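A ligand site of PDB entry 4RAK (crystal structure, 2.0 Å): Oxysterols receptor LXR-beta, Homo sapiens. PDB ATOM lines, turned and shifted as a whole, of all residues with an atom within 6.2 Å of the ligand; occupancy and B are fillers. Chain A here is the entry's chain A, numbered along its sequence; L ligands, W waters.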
ATOM      1  N   SER A  45       8.698  26.247   7.765  1.00  0.00           N
ATOM      2  CA  SER A  45       7.797  25.096   7.892  1.00  0.00           C
ATOM      3  C   SER A  45       8.059  23.976   6.877  1.00  0.00           C
ATOM      4  O   SER A  45       7.769  22.820   7.194  1.00  0.00           O
ATOM      5  CB  SER A  45       6.346  25.566   7.828  1.00  0.00           C
ATOM      6  OG  SER A  45       6.026  26.348   8.966  1.00  0.00           O
ATOM      7  N   PHE A  71      -5.111  10.960  10.287  1.00  0.00           N
ATOM      8  CA  PHE A  71      -5.512  11.794  11.400  1.00  0.00           C
ATOM      9  C   PHE A  71      -4.326  12.421  12.131  1.00  0.00           C
ATOM     10  O   PHE A  71      -4.340  13.634  12.394  1.00  0.00           O
ATOM     11  CB  PHE A  71      -6.396  11.004  12.376  1.00  0.00           C
ATOM     12  CG  PHE A  71      -6.902  11.806  13.539  1.00  0.00           C
ATOM     13  CD1 PHE A  71      -6.158  11.917  14.709  1.00  0.00           C
ATOM     14  CD2 PHE A  71      -8.129  12.459  13.482  1.00  0.00           C
ATOM     15  CE1 PHE A  71      -6.620  12.661  15.780  1.00  0.00           C
ATOM     16  CE2 PHE A  71      -8.597  13.209  14.548  1.00  0.00           C
ATOM     17  CZ  PHE A  71      -7.842  13.295  15.698  1.00  0.00           C
ATOM     18  N   PHE A  74      -2.706  15.204   9.928  1.00  0.00           N
ATOM     19  CA  PHE A  74      -3.490  16.438   9.939  1.00  0.00           C
ATOM     20  C   PHE A  74      -3.356  17.164  11.274  1.00  0.00           C
ATOM     21  O   PHE A  74      -3.378  18.394  11.292  1.00  0.00           O
ATOM     22  CB  PHE A  74      -4.973  16.163   9.632  1.00  0.00           C
ATOM     23  CG  PHE A  74      -5.317  16.152   8.165  1.00  0.00           C
ATOM     24  CD1 PHE A  74      -5.026  17.227   7.356  1.00  0.00           C
ATOM     25  CD2 PHE A  74      -6.006  15.088   7.623  1.00  0.00           C
ATOM     26  CE1 PHE A  74      -5.370  17.219   6.001  1.00  0.00           C
ATOM     27  CE2 PHE A  74      -6.363  15.084   6.267  1.00  0.00           C
ATOM     28  CZ  PHE A  74      -6.039  16.146   5.465  1.00  0.00           C
ATOM     29  N   THR A  75      -3.204  16.399  12.383  1.00  0.00           N
ATOM     30  CA  THR A  75      -2.953  16.914  13.741  1.00  0.00           C
ATOM     31  C   THR A  75      -1.617  17.629  13.756  1.00  0.00           C
ATOM     32  O   THR A  75      -1.505  18.723  14.319  1.00  0.00           O
ATOM     33  CB  THR A  75      -2.978  15.766  14.767  1.00  0.00           C
ATOM     34  OG1 THR A  75      -4.247  15.102  14.690  1.00  0.00           O
ATOM     35  CG2 THR A  75      -2.769  16.252  16.204  1.00  0.00           C
ATOM     36  N   GLU A  76      -0.605  17.029  13.107  1.00  0.00           N
ATOM     37  CA  GLU A  76       0.749  17.563  12.986  1.00  0.00           C
ATOM     38  C   GLU A  76       0.816  18.818  12.132  1.00  0.00           C
ATOM     39  O   GLU A  76       1.563  19.723  12.453  1.00  0.00           O
ATOM     40  CB  GLU A  76       1.712  16.502  12.455  1.00  0.00           C
ATOM     41  CG  GLU A  76       2.487  15.781  13.546  1.00  0.00           C
ATOM     42  CD  GLU A  76       2.926  14.369  13.199  1.00  0.00           C
ATOM     43  OE1 GLU A  76       4.090  14.021  13.504  1.00  0.00           O
ATOM     44  OE2 GLU A  76       2.093  13.595  12.660  1.00  0.00           O
ATOM     45  N   LEU A  77       0.056  18.852  11.034  1.00  0.00           N
ATOM     46  CA  LEU A  77      -0.051  19.998  10.118  1.00  0.00           C
ATOM     47  C   LEU A  77      -0.651  21.211  10.865  1.00  0.00           C
ATOM     48  O   LEU A  77      -0.195  22.339  10.678  1.00  0.00           O
ATOM     49  CB  LEU A  77      -0.895  19.600   8.897  1.00  0.00           C
ATOM     50  CG  LEU A  77      -0.170  19.251   7.568  1.00  0.00           C
ATOM     51  CD1 LEU A  77       1.156  18.538   7.785  1.00  0.00           C
ATOM     52  CD2 LEU A  77      -1.062  18.448   6.638  1.00  0.00           C
ATOM     53  N   ALA A  78      -1.617  20.931  11.782  1.00  0.00           N
ATOM     54  CA  ALA A  78      -2.239  21.930  12.650  1.00  0.00           C
ATOM     55  C   ALA A  78      -1.234  22.436  13.691  1.00  0.00           C
ATOM     56  O   ALA A  78      -1.251  23.619  14.014  1.00  0.00           O
ATOM     57  CB  ALA A  78      -3.460  21.355  13.335  1.00  0.00           C
ATOM     58  N   ILE A  80       1.997  22.605  13.301  1.00  0.00           N
ATOM     59  CA  ILE A  80       2.943  23.448  12.561  1.00  0.00           C
ATOM     60  C   ILE A  80       2.289  24.830  12.343  1.00  0.00           C
ATOM     61  O   ILE A  80       2.915  25.846  12.585  1.00  0.00           O
ATOM     62  CB  ILE A  80       3.421  22.764  11.254  1.00  0.00           C
ATOM     63  CG1 ILE A  80       4.228  21.480  11.578  1.00  0.00           C
ATOM     64  CG2 ILE A  80       4.271  23.736  10.429  1.00  0.00           C
ATOM     65  CD1 ILE A  80       4.247  20.461  10.429  1.00  0.00           C
ATOM     66  N   SER A  81       1.008  24.832  11.937  1.00  0.00           N
ATOM     67  CA  SER A  81       0.225  26.032  11.709  1.00  0.00           C
ATOM     68  C   SER A  81       0.260  26.950  12.908  1.00  0.00           C
ATOM     69  O   SER A  81       0.600  28.119  12.756  1.00  0.00           O
ATOM     70  CB  SER A  81      -1.202  25.693  11.328  1.00  0.00           C
ATOM     71  OG  SER A  81      -1.885  26.873  10.961  1.00  0.00           O
ATOM     72  N   VAL A  82       0.006  26.404  14.107  1.00  0.00           N
ATOM     73  CA  VAL A  82       0.034  27.182  15.350  1.00  0.00           C
ATOM     74  C   VAL A  82       1.339  27.936  15.531  1.00  0.00           C
ATOM     75  O   VAL A  82       1.317  29.127  15.831  1.00  0.00           O
ATOM     76  CB  VAL A  82      -0.322  26.342  16.619  1.00  0.00           C
ATOM     77  CG1 VAL A  82       0.052  27.084  17.899  1.00  0.00           C
ATOM     78  CG2 VAL A  82      -1.797  25.975  16.634  1.00  0.00           C
ATOM     79  N   GLU A  84       3.600  28.703  13.303  1.00  0.00           N
ATOM     80  CA  GLU A  84       3.671  29.615  12.179  1.00  0.00           C
ATOM     81  C   GLU A  84       2.860  30.877  12.466  1.00  0.00           C
ATOM     82  O   GLU A  84       3.319  31.982  12.159  1.00  0.00           O
ATOM     83  CB  GLU A  84       3.122  28.936  10.908  1.00  0.00           C
ATOM     84  CG  GLU A  84       3.899  29.208   9.642  1.00  0.00           C
ATOM     85  CD  GLU A  84       3.307  28.468   8.470  1.00  0.00           C
ATOM     86  OE1 GLU A  84       3.628  27.271   8.340  1.00  0.00           O
ATOM     87  OE2 GLU A  84       2.505  29.077   7.712  1.00  0.00           O
ATOM     88  N   ILE A 112      -7.797  29.597  15.070  1.00  0.00           N
ATOM     89  CA  ILE A 112      -8.714  28.860  14.205  1.00  0.00           C
ATOM     90  C   ILE A 112      -9.179  29.699  13.015  1.00  0.00           C
ATOM     91  O   ILE A 112      -9.281  29.175  11.900  1.00  0.00           O
ATOM     92  CB  ILE A 112      -9.858  28.232  15.060  1.00  0.00           C
ATOM     93  CG1 ILE A 112     -10.610  27.108  14.274  1.00  0.00           C
ATOM     94  CG2 ILE A 112     -10.782  29.261  15.661  1.00  0.00           C
ATOM     95  CD1 ILE A 112     -11.761  27.512  13.352  1.00  0.00           C
ATOM     96  N   ILE A 114      -7.441  32.211  11.671  1.00  0.00           N
ATOM     97  CA  ILE A 114      -6.228  32.359  10.831  1.00  0.00           C
ATOM     98  C   ILE A 114      -5.980  31.080  10.009  1.00  0.00           C
ATOM     99  O   ILE A 114      -5.722  31.172   8.811  1.00  0.00           O
ATOM    100  CB  ILE A 114      -5.010  32.833  11.626  1.00  0.00           C
ATOM    101  CG1 ILE A 114      -5.294  34.242  12.252  1.00  0.00           C
ATOM    102  CG2 ILE A 114      -3.779  32.871  10.696  1.00  0.00           C
ATOM    103  CD1 ILE A 114      -4.285  34.691  13.350  1.00  0.00           C
ATOM    104  N   MET A 115      -6.105  29.883  10.642  1.00  0.00           N
ATOM    105  CA  MET A 115      -5.976  28.578   9.980  1.00  0.00           C
ATOM    106  C   MET A 115      -6.902  28.487   8.776  1.00  0.00           C
ATOM    107  O   MET A 115      -6.511  28.033   7.709  1.00  0.00           O
ATOM    108  CB  MET A 115      -6.304  27.451  10.948  1.00  0.00           C
ATOM    109  CG  MET A 115      -5.207  27.097  11.872  1.00  0.00           C
ATOM    110  SD  MET A 115      -5.820  25.918  13.097  1.00  0.00           S
ATOM    111  CE  MET A 115      -4.356  25.620  13.960  1.00  0.00           C
ATOM    112  N   LEU A 116      -8.132  28.919   8.957  1.00  0.00           N
ATOM    113  CA  LEU A 116      -9.173  28.892   7.939  1.00  0.00           C
ATOM    114  C   LEU A 116      -8.851  29.872   6.791  1.00  0.00           C
ATOM    115  O   LEU A 116      -9.084  29.551   5.620  1.00  0.00           O
ATOM    116  CB  LEU A 116     -10.457  29.339   8.644  1.00  0.00           C
ATOM    117  CG  LEU A 116     -11.684  28.424   8.800  1.00  0.00           C
ATOM    118  CD1 LEU A 116     -11.357  26.952   8.820  1.00  0.00           C
ATOM    119  CD2 LEU A 116     -12.500  28.846  10.012  1.00  0.00           C
ATOM    120  N   GLU A 118      -5.819  31.042   6.006  1.00  0.00           N
ATOM    121  CA  GLU A 118      -4.627  30.449   5.405  1.00  0.00           C
ATOM    122  C   GLU A 118      -4.982  29.259   4.463  1.00  0.00           C
ATOM    123  O   GLU A 118      -4.374  29.118   3.416  1.00  0.00           O
ATOM    124  CB  GLU A 118      -3.634  30.036   6.492  1.00  0.00           C
ATOM    125  CG  GLU A 118      -2.298  29.531   5.995  1.00  0.00           C
ATOM    126  CD  GLU A 118      -1.372  30.515   5.273  1.00  0.00           C
ATOM    127  OE1 GLU A 118      -1.770  31.682   5.045  1.00  0.00           O
ATOM    128  OE2 GLU A 118      -0.251  30.097   4.924  1.00  0.00           O
ATOM    129  N   THR A 119      -5.973  28.455   4.841  1.00  0.00           N
ATOM    130  CA  THR A 119      -6.469  27.306   4.066  1.00  0.00           C
ATOM    131  C   THR A 119      -7.076  27.772   2.733  1.00  0.00           C
ATOM    132  O   THR A 119      -6.807  27.178   1.699  1.00  0.00           O
ATOM    133  CB  THR A 119      -7.444  26.470   4.933  1.00  0.00           C
ATOM    134  OG1 THR A 119      -6.693  25.891   6.012  1.00  0.00           O
ATOM    135  CG2 THR A 119      -8.148  25.366   4.161  1.00  0.00           C
ATOM    136  N   ARG A 122      -4.569  28.719   0.181  1.00  0.00           N
ATOM    137  CA  ARG A 122      -3.928  27.526  -0.349  1.00  0.00           C
ATOM    138  C   ARG A 122      -4.875  26.649  -1.167  1.00  0.00           C
ATOM    139  O   ARG A 122      -4.497  25.571  -1.614  1.00  0.00           O
ATOM    140  CB  ARG A 122      -3.261  26.764   0.802  1.00  0.00           C
ATOM    141  CG  ARG A 122      -2.094  27.519   1.391  1.00  0.00           C
ATOM    142  CD  ARG A 122      -1.615  27.011   2.745  1.00  0.00           C
ATOM    143  NE  ARG A 122      -0.165  26.826   2.721  1.00  0.00           N
ATOM    144  CZ  ARG A 122       0.651  27.043   3.743  1.00  0.00           C
ATOM    145  NH1 ARG A 122       0.186  27.432   4.917  1.00  0.00           N
ATOM    146  NH2 ARG A 122       1.950  26.861   3.599  1.00  0.00           N
ATOM    147  N   THR A 131      -3.503  22.877  -0.608  1.00  0.00           N
ATOM    148  CA  THR A 131      -2.079  22.569  -0.458  1.00  0.00           C
ATOM    149  C   THR A 131      -1.585  22.950   0.923  1.00  0.00           C
ATOM    150  O   THR A 131      -1.501  24.134   1.257  1.00  0.00           O
ATOM    151  CB  THR A 131      -1.255  23.213  -1.579  1.00  0.00           C
ATOM    152  OG1 THR A 131      -1.673  22.640  -2.821  1.00  0.00           O
ATOM    153  CG2 THR A 131       0.259  23.020  -1.404  1.00  0.00           C
ATOM    154  N   PHE A 132      -1.282  21.959   1.735  1.00  0.00           N
ATOM    155  CA  PHE A 132      -0.718  22.213   3.047  1.00  0.00           C
ATOM    156  C   PHE A 132       0.774  22.138   2.891  1.00  0.00           C
ATOM    157  O   PHE A 132       1.278  21.365   2.072  1.00  0.00           O
ATOM    158  CB  PHE A 132      -1.301  21.277   4.122  1.00  0.00           C
ATOM    159  CG  PHE A 132      -2.717  21.622   4.494  1.00  0.00           C
ATOM    160  CD1 PHE A 132      -3.081  22.935   4.800  1.00  0.00           C
ATOM    161  CD2 PHE A 132      -3.703  20.646   4.543  1.00  0.00           C
ATOM    162  CE1 PHE A 132      -4.392  23.255   5.150  1.00  0.00           C
ATOM    163  CE2 PHE A 132      -5.006  20.962   4.882  1.00  0.00           C
ATOM    164  CZ  PHE A 132      -5.346  22.260   5.200  1.00  0.00           C
ATOM    165  N   LEU A 133       1.492  22.907   3.699  1.00  0.00           N
ATOM    166  CA  LEU A 133       2.905  23.158   3.469  1.00  0.00           C
ATOM    167  C   LEU A 133       2.961  23.694   2.055  1.00  0.00           C
ATOM    168  O   LEU A 133       2.100  24.493   1.716  1.00  0.00           O
ATOM    169  CB  LEU A 133       3.752  21.913   3.673  1.00  0.00           C
ATOM    170  CG  LEU A 133       4.323  21.726   5.088  1.00  0.00           C
ATOM    171  CD1 LEU A 133       4.178  22.915   6.014  1.00  0.00           C
ATOM    172  CD2 LEU A 133       3.834  20.486   5.796  1.00  0.00           C
ATOM    173  N   LYS A 134       3.923  23.298   1.237  1.00  0.00           N
ATOM    174  CA  LYS A 134       3.784  23.659  -0.168  1.00  0.00           C
ATOM    175  C   LYS A 134       3.837  22.527  -1.137  1.00  0.00           C
ATOM    176  O   LYS A 134       3.670  22.737  -2.326  1.00  0.00           O
ATOM    177  CB  LYS A 134       4.635  24.854  -0.575  1.00  0.00           C
ATOM    178  CG  LYS A 134       3.808  25.925  -1.324  1.00  0.00           C
ATOM    179  CD  LYS A 134       3.267  27.016  -0.376  1.00  0.00           C
ATOM    180  CE  LYS A 134       2.290  27.882  -1.122  1.00  0.00           C
ATOM    181  NZ  LYS A 134       1.783  29.062  -0.357  1.00  0.00           N
ATOM    182  N   PHE A 143      -9.991  14.542   3.487  1.00  0.00           N
ATOM    183  CA  PHE A 143     -10.336  14.995   4.834  1.00  0.00           C
ATOM    184  C   PHE A 143     -11.359  14.030   5.438  1.00  0.00           C
ATOM    185  O   PHE A 143     -11.266  13.685   6.618  1.00  0.00           O
ATOM    186  CB  PHE A 143     -10.873  16.438   4.807  1.00  0.00           C
ATOM    187  CG  PHE A 143      -9.854  17.478   4.401  1.00  0.00           C
ATOM    188  CD1 PHE A 143      -9.019  18.068   5.342  1.00  0.00           C
ATOM    189  CD2 PHE A 143      -9.731  17.862   3.073  1.00  0.00           C
ATOM    190  CE1 PHE A 143      -8.087  19.025   4.963  1.00  0.00           C
ATOM    191  CE2 PHE A 143      -8.792  18.816   2.682  1.00  0.00           C
ATOM    192  CZ  PHE A 143      -7.969  19.385   3.631  1.00  0.00           C
ATOM    193  N   LEU A 148     -12.319  13.147   9.605  1.00  0.00           N
ATOM    194  CA  LEU A 148     -12.677  14.493  10.033  1.00  0.00           C
ATOM    195  C   LEU A 148     -14.176  14.614   9.815  1.00  0.00           C
ATOM    196  O   LEU A 148     -14.741  13.924   8.945  1.00  0.00           O
ATOM    197  CB  LEU A 148     -11.938  15.555   9.221  1.00  0.00           C
ATOM    198  CG  LEU A 148     -10.572  16.061   9.672  1.00  0.00           C
ATOM    199  CD1 LEU A 148      -9.883  15.106  10.598  1.00  0.00           C
ATOM    200  CD2 LEU A 148      -9.704  16.304   8.464  1.00  0.00           C
ATOM    201  N   PHE A 152     -17.903  20.175   9.436  1.00  0.00           N
ATOM    202  CA  PHE A 152     -16.901  21.221   9.398  1.00  0.00           C
ATOM    203  C   PHE A 152     -16.065  21.179   8.113  1.00  0.00           C
ATOM    204  O   PHE A 152     -15.582  22.228   7.700  1.00  0.00           O
ATOM    205  CB  PHE A 152     -16.008  21.214  10.649  1.00  0.00           C
ATOM    206  CG  PHE A 152     -15.213  22.481  10.867  1.00  0.00           C
ATOM    207  CD1 PHE A 152     -15.844  23.713  11.070  1.00  0.00           C
ATOM    208  CD2 PHE A 152     -13.829  22.440  10.909  1.00  0.00           C
ATOM    209  CE1 PHE A 152     -15.101  24.875  11.274  1.00  0.00           C
ATOM    210  CE2 PHE A 152     -13.093  23.606  11.125  1.00  0.00           C
ATOM    211  CZ  PHE A 152     -13.730  24.807  11.317  1.00  0.00           C
ATOM    212  N   ILE A 153     -15.951  20.002   7.466  1.00  0.00           N
ATOM    213  CA  ILE A 153     -15.196  19.864   6.206  1.00  0.00           C
ATOM    214  C   ILE A 153     -15.873  20.646   5.051  1.00  0.00           C
ATOM    215  O   ILE A 153     -15.200  21.392   4.340  1.00  0.00           O
ATOM    216  CB  ILE A 153     -14.905  18.377   5.845  1.00  0.00           C
ATOM    217  CG1 ILE A 153     -14.014  17.739   6.918  1.00  0.00           C
ATOM    218  CG2 ILE A 153     -14.259  18.234   4.449  1.00  0.00           C
ATOM    219  CD1 ILE A 153     -14.166  16.234   7.008  1.00  0.00           C
ATOM    220  N   ILE A 156     -15.432  24.437   5.377  1.00  0.00           N
ATOM    221  CA  ILE A 156     -14.042  24.805   5.032  1.00  0.00           C
ATOM    222  C   ILE A 156     -13.913  25.002   3.520  1.00  0.00           C
ATOM    223  O   ILE A 156     -13.336  26.009   3.076  1.00  0.00           O
ATOM    224  CB  ILE A 156     -13.007  23.784   5.580  1.00  0.00           C
ATOM    225  CG1 ILE A 156     -12.925  23.847   7.109  1.00  0.00           C
ATOM    226  CG2 ILE A 156     -11.618  24.003   4.956  1.00  0.00           C
ATOM    227  CD1 ILE A 156     -12.134  22.740   7.744  1.00  0.00           C
ATOM    228  N   HIS A 238     -17.066  25.472  15.353  1.00  0.00           N
ATOM    229  CA  HIS A 238     -16.036  24.440  15.512  1.00  0.00           C
ATOM    230  C   HIS A 238     -15.842  24.082  16.976  1.00  0.00           C
ATOM    231  O   HIS A 238     -15.601  22.930  17.302  1.00  0.00           O
ATOM    232  CB  HIS A 238     -14.711  24.890  14.908  1.00  0.00           C
ATOM    233  CG  HIS A 238     -13.617  23.874  15.041  1.00  0.00           C
ATOM    234  ND1 HIS A 238     -12.644  23.973  16.028  1.00  0.00           N
ATOM    235  CD2 HIS A 238     -13.391  22.729  14.359  1.00  0.00           C
ATOM    236  CE1 HIS A 238     -11.853  22.919  15.890  1.00  0.00           C
ATOM    237  NE2 HIS A 238     -12.267  22.149  14.890  1.00  0.00           N
HETATM  238  C1  LIG L   1       1.437  24.703   8.382  1.00  0.00           C
HETATM  239  S1  LIG L   1       0.288  24.052   7.153  1.00  0.00           S
HETATM  240  O1  LIG L   1       0.643  24.628   5.636  1.00  0.00           O
HETATM  241  O2  LIG L   1       0.351  22.398   7.115  1.00  0.00           O
HETATM  242  C2  LIG L   1      -1.420  24.544   7.511  1.00  0.00           C
HETATM  243  C3  LIG L   1      -2.207  23.661   8.250  1.00  0.00           C
HETATM  244  C4  LIG L   1      -1.912  25.771   7.064  1.00  0.00           C
HETATM  245  C5  LIG L   1      -3.225  26.127   7.350  1.00  0.00           C
HETATM  246  C6  LIG L   1      -4.032  25.247   8.075  1.00  0.00           C
HETATM  247  C7  LIG L   1      -3.518  24.025   8.542  1.00  0.00           C
HETATM  248  C8  LIG L   1      -4.408  23.061   9.323  1.00  0.00           C
HETATM  249  C9  LIG L   1      -5.034  23.472  10.501  1.00  0.00           C
HETATM  250  C10 LIG L   1      -5.844  22.573  11.188  1.00  0.00           C
HETATM  251  C11 LIG L   1      -4.588  21.764   8.847  1.00  0.00           C
HETATM  252  C12 LIG L   1      -5.400  20.856   9.545  1.00  0.00           C
HETATM  253  C13 LIG L   1      -6.033  21.267  10.710  1.00  0.00           C
HETATM  254  N1  LIG L   1      -6.927  20.359  11.434  1.00  0.00           N
HETATM  255  C14 LIG L   1      -6.588  19.659  12.490  1.00  0.00           C
HETATM  256  C15 LIG L   1      -7.701  18.933  12.895  1.00  0.00           C
HETATM  257  C16 LIG L   1      -7.784  17.952  14.061  1.00  0.00           C
HETATM  258  C17 LIG L   1      -8.597  16.738  13.649  1.00  0.00           C
HETATM  259  C18 LIG L   1      -8.445  18.628  15.249  1.00  0.00           C
HETATM  260  O3  LIG L   1      -6.500  17.545  14.434  1.00  0.00           O
HETATM  261  N2  LIG L   1      -8.680  19.263  12.062  1.00  0.00           N
HETATM  262  C19 LIG L   1      -8.222  20.117  11.162  1.00  0.00           C
HETATM  263  C20 LIG L   1      -9.076  20.671  10.010  1.00  0.00           C
HETATM  264  C21 LIG L   1      -8.695  19.892   8.744  1.00  0.00           C
HETATM  265  C22 LIG L   1     -10.571  20.409  10.236  1.00  0.00           C
HETATM  266  C23 LIG L   1      -8.884  22.199   9.834  1.00  0.00           C
HETATM  267  C24 LIG L   1      -8.560  22.715   8.569  1.00  0.00           C
HETATM  268  C25 LIG L   1      -8.379  24.063   8.361  1.00  0.00           C
HETATM  269  C26 LIG L   1      -8.516  24.949   9.421  1.00  0.00           C
HETATM  270  C27 LIG L   1      -8.840  24.470  10.691  1.00  0.00           C
HETATM  271  C28 LIG L   1      -9.033  23.102  10.907  1.00  0.00           C
HETATM  272 CL1  LIG L   1      -9.404  22.572  12.582  1.00  0.00          CL
HETATM  273  O   HOH W   1     -11.522  19.001  13.357  1.00  0.00           O
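An oxygen (O1) of the ligand is in hydrogen-bond range of the guanidinium group of Arg 122 (2.9 Å). The backbone NH (N) of Leu 133 lies within hydrogen-bond range of an oxygen (O1) of the ligand. The side-chain hydroxyl (OG1) of Thr 75 sits at hydrogen-bond distance from an oxygen (O3) of the ligand (3.3 Å).
The guanidinium group of Arg 122 sits at hydrogen-bond distance from the backbone carbonyl oxygen of Leu 133 (3.0 Å). The backbone NH (N) of Leu 148 lies within hydrogen-bond range of the backbone carbonyl oxygen (O) of Phe 143, 3.2 Å away. NH1 of Arg 122 is in salt-bridge range of OE2 of Glu 84 (3.99 Å). O of Arg 122 lies within hydrogen-bond range of N of Thr 131. OG1 of Thr 119 sits at hydrogen-bond distance from O of Met 115 (2.7 Å). NH1 of Arg 122 is in salt-bridge range of OE2 of Glu 118, 2.7 Å away. OG1 of Thr 75 is in hydrogen-bond range of O of Phe 71 (2.7 Å). The side-chain hydroxyl (OG) of Ser 45 is in hydrogen-bond range of the side-chain carboxylate (OE1) of Glu 84, at 2.6 Å.
Merely in contact with the ligand: Phe 71, Phe 74, Leu 77, Ala 78, Ile 80, Ser 81, Glu 84, Met 115, Leu 116, Glu 118, Thr 119, Phe 132, Phe 143, Leu 148, Phe 152, Ile 156 and His 238. Hydrophobic or aromatic side chains within 4 Å of the ligand: Phe 71, Leu 77, Ala 78, Ile 80, Met 115, Leu 116, Phe 132, Leu 133, Phe 143, Leu 148, Phe 152 and Ile 156. Of the 28 residues printed, 20 come within 4 Å of the ligand.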
